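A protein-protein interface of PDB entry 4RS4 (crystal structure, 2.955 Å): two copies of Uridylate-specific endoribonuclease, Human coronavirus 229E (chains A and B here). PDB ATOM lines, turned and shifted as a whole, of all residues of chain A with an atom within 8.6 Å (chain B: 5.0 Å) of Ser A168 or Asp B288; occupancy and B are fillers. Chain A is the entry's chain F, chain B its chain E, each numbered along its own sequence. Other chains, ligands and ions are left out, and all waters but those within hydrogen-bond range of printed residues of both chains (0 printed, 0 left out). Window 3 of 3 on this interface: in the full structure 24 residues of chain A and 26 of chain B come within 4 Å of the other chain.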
ATOM      1  N   LEU A 158      11.156  16.209 -16.174  1.00  0.00           N
ATOM      2  CA  LEU A 158      10.911  15.431 -17.378  1.00  0.00           C
ATOM      3  C   LEU A 158      11.826  14.211 -17.386  1.00  0.00           C
ATOM      4  O   LEU A 158      13.043  14.336 -17.536  1.00  0.00           O
ATOM      5  CB  LEU A 158      11.135  16.283 -18.631  1.00  0.00           C
ATOM      6  CG  LEU A 158      10.869  15.597 -19.970  1.00  0.00           C
ATOM      7  CD1 LEU A 158       9.548  14.846 -19.925  1.00  0.00           C
ATOM      8  CD2 LEU A 158      10.868  16.624 -21.083  1.00  0.00           C
ATOM      9  N   ILE A 163      13.197  20.511 -15.724  1.00  0.00           N
ATOM     10  CA  ILE A 163      12.827  21.403 -16.820  1.00  0.00           C
ATOM     11  C   ILE A 163      12.017  22.589 -16.303  1.00  0.00           C
ATOM     12  O   ILE A 163      11.747  22.692 -15.104  1.00  0.00           O
ATOM     13  CB  ILE A 163      12.010  20.670 -17.903  1.00  0.00           C
ATOM     14  CG1 ILE A 163      10.663  20.217 -17.340  1.00  0.00           C
ATOM     15  CG2 ILE A 163      12.789  19.487 -18.449  1.00  0.00           C
ATOM     16  CD1 ILE A 163       9.828  19.419 -18.321  1.00  0.00           C
ATOM     17  N   ALA A 164      11.611  23.470 -17.212  1.00  0.00           N
ATOM     18  CA  ALA A 164      10.905  24.682 -16.823  1.00  0.00           C
ATOM     19  C   ALA A 164      10.452  25.495 -18.022  1.00  0.00           C
ATOM     20  O   ALA A 164      10.891  25.260 -19.146  1.00  0.00           O
ATOM     21  CB  ALA A 164      11.777  25.537 -15.917  1.00  0.00           C
ATOM     22  N   THR A 165       9.562  26.446 -17.768  1.00  0.00           N
ATOM     23  CA  THR A 165       9.085  27.344 -18.806  1.00  0.00           C
ATOM     24  C   THR A 165      10.256  28.099 -19.432  1.00  0.00           C
ATOM     25  O   THR A 165      11.126  28.603 -18.724  1.00  0.00           O
ATOM     26  CB  THR A 165       8.066  28.344 -18.247  1.00  0.00           C
ATOM     27  OG1 THR A 165       6.958  27.632 -17.681  1.00  0.00           O
ATOM     28  CG2 THR A 165       7.571  29.264 -19.348  1.00  0.00           C
ATOM     29  N   VAL A 166      10.271  28.158 -20.761  1.00  0.00           N
ATOM     30  CA  VAL A 166      11.352  28.801 -21.506  1.00  0.00           C
ATOM     31  C   VAL A 166      10.819  29.504 -22.756  1.00  0.00           C
ATOM     32  O   VAL A 166       9.815  29.080 -23.332  1.00  0.00           O
ATOM     33  CB  VAL A 166      12.419  27.775 -21.915  1.00  0.00           C
ATOM     34  CG1 VAL A 166      13.260  27.364 -20.718  1.00  0.00           C
ATOM     35  CG2 VAL A 166      11.755  26.560 -22.545  1.00  0.00           C
ATOM     36  N   LYS A 167      11.488  30.582 -23.164  1.00  0.00           N
ATOM     37  CA  LYS A 167      11.083  31.359 -24.337  1.00  0.00           C
ATOM     38  C   LYS A 167      11.504  30.721 -25.666  1.00  0.00           C
ATOM     39  O   LYS A 167      10.821  30.865 -26.685  1.00  0.00           O
ATOM     40  CB  LYS A 167      11.612  32.795 -24.225  1.00  0.00           C
ATOM     41  CG  LYS A 167      11.298  33.703 -25.419  1.00  0.00           C
ATOM     42  CD  LYS A 167       9.817  33.685 -25.774  1.00  0.00           C
ATOM     43  CE  LYS A 167       9.422  34.910 -26.592  1.00  0.00           C
ATOM     44  NZ  LYS A 167      10.030  36.156 -26.053  1.00  0.00           N
ATOM     45  N   SER A 168      12.621  29.999 -25.637  1.00  0.00           N
ATOM     46  CA  SER A 168      13.198  29.388 -26.839  1.00  0.00           C
ATOM     47  C   SER A 168      13.829  30.409 -27.800  1.00  0.00           C
ATOM     48  O   SER A 168      14.372  30.036 -28.846  1.00  0.00           O
ATOM     49  CB  SER A 168      12.187  28.491 -27.574  1.00  0.00           C
ATOM     50  OG  SER A 168      11.542  29.183 -28.629  1.00  0.00           O
ATOM     51  N   GLU A 169      13.739  31.691 -27.449  1.00  0.00           N
ATOM     52  CA  GLU A 169      14.441  32.749 -28.180  1.00  0.00           C
ATOM     53  C   GLU A 169      14.073  32.785 -29.664  1.00  0.00           C
ATOM     54  O   GLU A 169      12.931  33.081 -30.019  1.00  0.00           O
ATOM     55  CB  GLU A 169      15.950  32.571 -28.026  1.00  0.00           C
ATOM     56  CG  GLU A 169      16.766  33.826 -28.250  1.00  0.00           C
ATOM     57  CD  GLU A 169      18.222  33.506 -28.499  1.00  0.00           C
ATOM     58  OE1 GLU A 169      18.499  32.406 -29.019  1.00  0.00           O
ATOM     59  OE2 GLU A 169      19.089  34.342 -28.169  1.00  0.00           O
ATOM     60  N   ASP A 170      15.060  32.521 -30.520  1.00  0.00           N
ATOM     61  CA  ASP A 170      14.873  32.465 -31.971  1.00  0.00           C
ATOM     62  C   ASP A 170      13.776  31.483 -32.383  1.00  0.00           C
ATOM     63  O   ASP A 170      12.590  31.705 -32.146  1.00  0.00           O
ATOM     64  CB  ASP A 170      16.184  32.058 -32.659  1.00  0.00           C
ATOM     65  CG  ASP A 170      17.099  33.239 -32.953  1.00  0.00           C
ATOM     66  OD1 ASP A 170      16.677  34.403 -32.765  1.00  0.00           O
ATOM     67  OD2 ASP A 170      18.242  32.990 -33.397  1.00  0.00           O
ATOM     68  N   ASN A 172       6.725  30.527 -29.736  1.00  0.00           N
ATOM     69  CA  ASN A 172       7.957  29.809 -29.422  1.00  0.00           C
ATOM     70  C   ASN A 172       8.103  29.499 -27.931  1.00  0.00           C
ATOM     71  O   ASN A 172       9.099  28.919 -27.505  1.00  0.00           O
ATOM     72  CB  ASN A 172       9.183  30.571 -29.936  1.00  0.00           C
ATOM     73  CG  ASN A 172       9.327  31.949 -29.309  1.00  0.00           C
ATOM     74  OD1 ASN A 172       8.340  32.639 -29.059  1.00  0.00           O
ATOM     75  ND2 ASN A 172      10.566  32.353 -29.051  1.00  0.00           N
ATOM     76  N   ILE A 173       7.098  29.873 -27.144  1.00  0.00           N
ATOM     77  CA  ILE A 173       7.096  29.586 -25.707  1.00  0.00           C
ATOM     78  C   ILE A 173       6.995  28.079 -25.437  1.00  0.00           C
ATOM     79  O   ILE A 173       6.580  27.309 -26.313  1.00  0.00           O
ATOM     80  CB  ILE A 173       5.945  30.330 -24.972  1.00  0.00           C
ATOM     81  CG1 ILE A 173       4.591  30.024 -25.621  1.00  0.00           C
ATOM     82  CG2 ILE A 173       6.195  31.837 -24.925  1.00  0.00           C
ATOM     83  CD1 ILE A 173       3.963  28.731 -25.135  1.00  0.00           C
ATOM     84  N   LYS A 174       7.427  27.655 -24.253  1.00  0.00           N
ATOM     85  CA  LYS A 174       7.176  26.291 -23.806  1.00  0.00           C
ATOM     86  C   LYS A 174       6.697  26.339 -22.360  1.00  0.00           C
ATOM     87  O   LYS A 174       7.463  26.707 -21.457  1.00  0.00           O
ATOM     88  CB  LYS A 174       8.437  25.431 -23.944  1.00  0.00           C
ATOM     89  CG  LYS A 174       8.166  23.985 -24.385  1.00  0.00           C
ATOM     90  CD  LYS A 174       9.040  23.628 -25.590  1.00  0.00           C
ATOM     91  CE  LYS A 174       8.782  22.215 -26.075  1.00  0.00           C
ATOM     92  NZ  LYS A 174       9.670  21.872 -27.212  1.00  0.00           N
ATOM     93  N   ASN A 175       5.449  25.939 -22.127  1.00  0.00           N
ATOM     94  CA  ASN A 175       4.890  26.064 -20.793  1.00  0.00           C
ATOM     95  C   ASN A 175       4.865  24.757 -20.008  1.00  0.00           C
ATOM     96  O   ASN A 175       4.170  23.801 -20.371  1.00  0.00           O
ATOM     97  CB  ASN A 175       3.505  26.708 -20.839  1.00  0.00           C
ATOM     98  CG  ASN A 175       3.544  28.191 -20.503  1.00  0.00           C
ATOM     99  OD1 ASN A 175       3.365  28.586 -19.347  1.00  0.00           O
ATOM    100  ND2 ASN A 175       3.788  29.017 -21.512  1.00  0.00           N
ATOM    101  N   ILE A 176       5.635  24.726 -18.925  1.00  0.00           N
ATOM    102  CA  ILE A 176       5.500  23.676 -17.929  1.00  0.00           C
ATOM    103  C   ILE A 176       4.710  24.267 -16.771  1.00  0.00           C
ATOM    104  O   ILE A 176       5.029  25.349 -16.281  1.00  0.00           O
ATOM    105  CB  ILE A 176       6.863  23.168 -17.433  1.00  0.00           C
ATOM    106  CG1 ILE A 176       7.818  22.975 -18.613  1.00  0.00           C
ATOM    107  CG2 ILE A 176       6.693  21.864 -16.657  1.00  0.00           C
ATOM    108  CD1 ILE A 176       7.370  21.903 -19.590  1.00  0.00           C
ATOM    109  N   LEU A 206      20.641  24.731 -15.499  1.00  0.00           N
ATOM    110  CA  LEU A 206      20.431  25.811 -16.455  1.00  0.00           C
ATOM    111  C   LEU A 206      19.736  26.982 -15.750  1.00  0.00           C
ATOM    112  O   LEU A 206      18.832  26.775 -14.938  1.00  0.00           O
ATOM    113  CB  LEU A 206      19.594  25.315 -17.638  1.00  0.00           C
ATOM    114  CG  LEU A 206      20.263  24.271 -18.540  1.00  0.00           C
ATOM    115  CD1 LEU A 206      19.252  23.513 -19.403  1.00  0.00           C
ATOM    116  CD2 LEU A 206      21.325  24.934 -19.404  1.00  0.00           C
ATOM    117  N   VAL B 242      13.354  20.180 -31.656  1.00  0.00           N
ATOM    118  CA  VAL B 242      13.250  20.465 -30.231  1.00  0.00           C
ATOM    119  C   VAL B 242      12.196  21.515 -29.893  1.00  0.00           C
ATOM    120  O   VAL B 242      11.996  21.828 -28.725  1.00  0.00           O
ATOM    121  CB  VAL B 242      14.593  20.957 -29.667  1.00  0.00           C
ATOM    122  CG1 VAL B 242      15.654  19.878 -29.787  1.00  0.00           C
ATOM    123  CG2 VAL B 242      15.021  22.227 -30.392  1.00  0.00           C
ATOM    124  N   SER B 243      11.527  22.058 -30.906  1.00  0.00           N
ATOM    125  CA  SER B 243      10.553  23.124 -30.687  1.00  0.00           C
ATOM    126  C   SER B 243       9.182  22.580 -30.310  1.00  0.00           C
ATOM    127  O   SER B 243       8.235  23.347 -30.123  1.00  0.00           O
ATOM    128  CB  SER B 243      10.455  24.018 -31.921  1.00  0.00           C
ATOM    129  OG  SER B 243      10.515  23.244 -33.110  1.00  0.00           O
ATOM    130  N   TYR B 285      15.625  16.455 -23.770  1.00  0.00           N
ATOM    131  CA  TYR B 285      16.405  17.657 -24.063  1.00  0.00           C
ATOM    132  C   TYR B 285      15.926  18.814 -23.178  1.00  0.00           C
ATOM    133  O   TYR B 285      14.784  19.260 -23.289  1.00  0.00           O
ATOM    134  CB  TYR B 285      16.299  18.010 -25.548  1.00  0.00           C
ATOM    135  CG  TYR B 285      17.123  19.203 -25.978  1.00  0.00           C
ATOM    136  CD1 TYR B 285      18.492  19.088 -26.198  1.00  0.00           C
ATOM    137  CD2 TYR B 285      16.529  20.440 -26.187  1.00  0.00           C
ATOM    138  CE1 TYR B 285      19.246  20.180 -26.600  1.00  0.00           C
ATOM    139  CE2 TYR B 285      17.271  21.534 -26.588  1.00  0.00           C
ATOM    140  CZ  TYR B 285      18.629  21.402 -26.793  1.00  0.00           C
ATOM    141  OH  TYR B 285      19.364  22.498 -27.192  1.00  0.00           O
ATOM    142  N   LEU B 286      16.807  19.288 -22.301  1.00  0.00           N
ATOM    143  CA  LEU B 286      16.435  20.227 -21.243  1.00  0.00           C
ATOM    144  C   LEU B 286      16.218  21.676 -21.703  1.00  0.00           C
ATOM    145  O   LEU B 286      15.239  22.312 -21.314  1.00  0.00           O
ATOM    146  CB  LEU B 286      17.478  20.195 -20.112  1.00  0.00           C
ATOM    147  CG  LEU B 286      17.466  19.059 -19.083  1.00  0.00           C
ATOM    148  CD1 LEU B 286      17.675  17.710 -19.737  1.00  0.00           C
ATOM    149  CD2 LEU B 286      18.528  19.292 -18.013  1.00  0.00           C
ATOM    150  N   ASN B 287      17.133  22.195 -22.516  1.00  0.00           N
ATOM    151  CA  ASN B 287      17.156  23.619 -22.858  1.00  0.00           C
ATOM    152  C   ASN B 287      15.871  24.161 -23.495  1.00  0.00           C
ATOM    153  O   ASN B 287      15.477  25.300 -23.230  1.00  0.00           O
ATOM    154  CB  ASN B 287      18.361  23.919 -23.752  1.00  0.00           C
ATOM    155  CG  ASN B 287      19.680  23.524 -23.103  1.00  0.00           C
ATOM    156  OD1 ASN B 287      20.000  22.339 -22.986  1.00  0.00           O
ATOM    157  ND2 ASN B 287      20.451  24.519 -22.681  1.00  0.00           N
ATOM    158  N   ASP B 288      15.244  23.349 -24.346  1.00  0.00           N
ATOM    159  CA  ASP B 288      13.950  23.653 -24.961  1.00  0.00           C
ATOM    160  C   ASP B 288      13.150  22.367 -24.779  1.00  0.00           C
ATOM    161  O   ASP B 288      13.027  21.571 -25.719  1.00  0.00           O
ATOM    162  CB  ASP B 288      14.134  23.972 -26.452  1.00  0.00           C
ATOM    163  CG  ASP B 288      12.925  24.671 -27.074  1.00  0.00           C
ATOM    164  OD1 ASP B 288      11.781  24.468 -26.607  1.00  0.00           O
ATOM    165  OD2 ASP B 288      13.135  25.425 -28.049  1.00  0.00           O
ATOM    166  N   PRO B 289      12.614  22.149 -23.562  1.00  0.00           N
ATOM    167  CA  PRO B 289      12.324  20.777 -23.127  1.00  0.00           C
ATOM    168  C   PRO B 289      11.494  19.956 -24.098  1.00  0.00           C
ATOM    169  O   PRO B 289      10.397  20.351 -24.482  1.00  0.00           O
ATOM    170  CB  PRO B 289      11.560  20.975 -21.805  1.00  0.00           C
ATOM    171  CG  PRO B 289      11.049  22.376 -21.850  1.00  0.00           C
ATOM    172  CD  PRO B 289      12.132  23.137 -22.581  1.00  0.00           C
ATOM    173  N   SER B 290      12.027  18.790 -24.446  1.00  0.00           N
ATOM    174  CA  SER B 290      11.397  17.883 -25.388  1.00  0.00           C
ATOM    175  C   SER B 290      11.837  16.462 -25.066  1.00  0.00           C
ATOM    176  O   SER B 290      12.920  16.246 -24.514  1.00  0.00           O
ATOM    177  CB  SER B 290      11.803  18.241 -26.815  1.00  0.00           C
ATOM    178  OG  SER B 290      11.086  17.467 -27.767  1.00  0.00           O
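NZ of Lys A174 sits at hydrogen-bond distance from O of Val B242. The side-chain carboxylate of Asp B288 lies within salt-bridge range of the side-chain amino group of Lys A174, 3.4 Å away. The backbone carbonyl oxygen (O) of Pro B289 lies close to the side-chain amino group (NZ) of Lys A174, 3.2 Å away.
The backbone NH (N) of Lys A174 is in hydrogen-bond range of the backbone carbonyl oxygen (O) of Val A166, at 2.9 Å. The backbone carbonyl oxygen (O) of Asn A172 is in hydrogen-bond range of the side-chain hydroxyl (OG) of Ser A168, at 2.7 Å.
Among the printed residues, pairs that only touch across the chains: Ile A163 with Pro B289, Ala A164 with Pro B289, Val A166 with Asn B287, Val A166 with Pro B289, Ser A168 with Asp B288, Lys A174 with Ser B243, Leu A206 with Leu B286 and Leu A206 with Asn B287.
Of the printed residues of chain B, Ser A168 touches Asp B288 (3.2 Å). Of chain A, only Ile A163 (3.9 Å), Ala A164 (3.96 Å), Val A166 (3.4 Å) and Lys A174 (2.9 Å) come within 4 Å of Pro B289. Printed residues of chain A within 4 Å of Asn B287: Val A166 (3.9 Å) and Leu A206 (3.4 Å). Of the printed residues of chain B, Val A166 touches Asn B287 and Pro B289. Lys A167 touches none of the printed residues of chain B. Ser B290 touches none of the printed residues of chain A.
Of the 15 printed residues of chain A, 6 touch a printed residue of chain B. Printed residues of chain A that touch a printed residue of chain B: Ile A163, Ala A164, Val A166, Ser A168, Lys A174 and Leu A206. Hydrophobic or aromatic side chains of chain A within 4 Å of the printed part of chain B: Ile A163, Val A166 and Leu A206. Along chain A the printed residues that touch a printed residue of chain B span positions 163 to 206. Printed residues of chain B that touch a printed residue of chain A: Val B242, Ser B243, Leu B286, Asn B287, Asp B288 and Pro B289. Hydrophobic or aromatic side chains of chain B within 4 Å of the printed part of chain A: Leu B286 and Pro B289. Among the printed residues, 11 pairs touch across the chains.
No position is printed for both chains.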
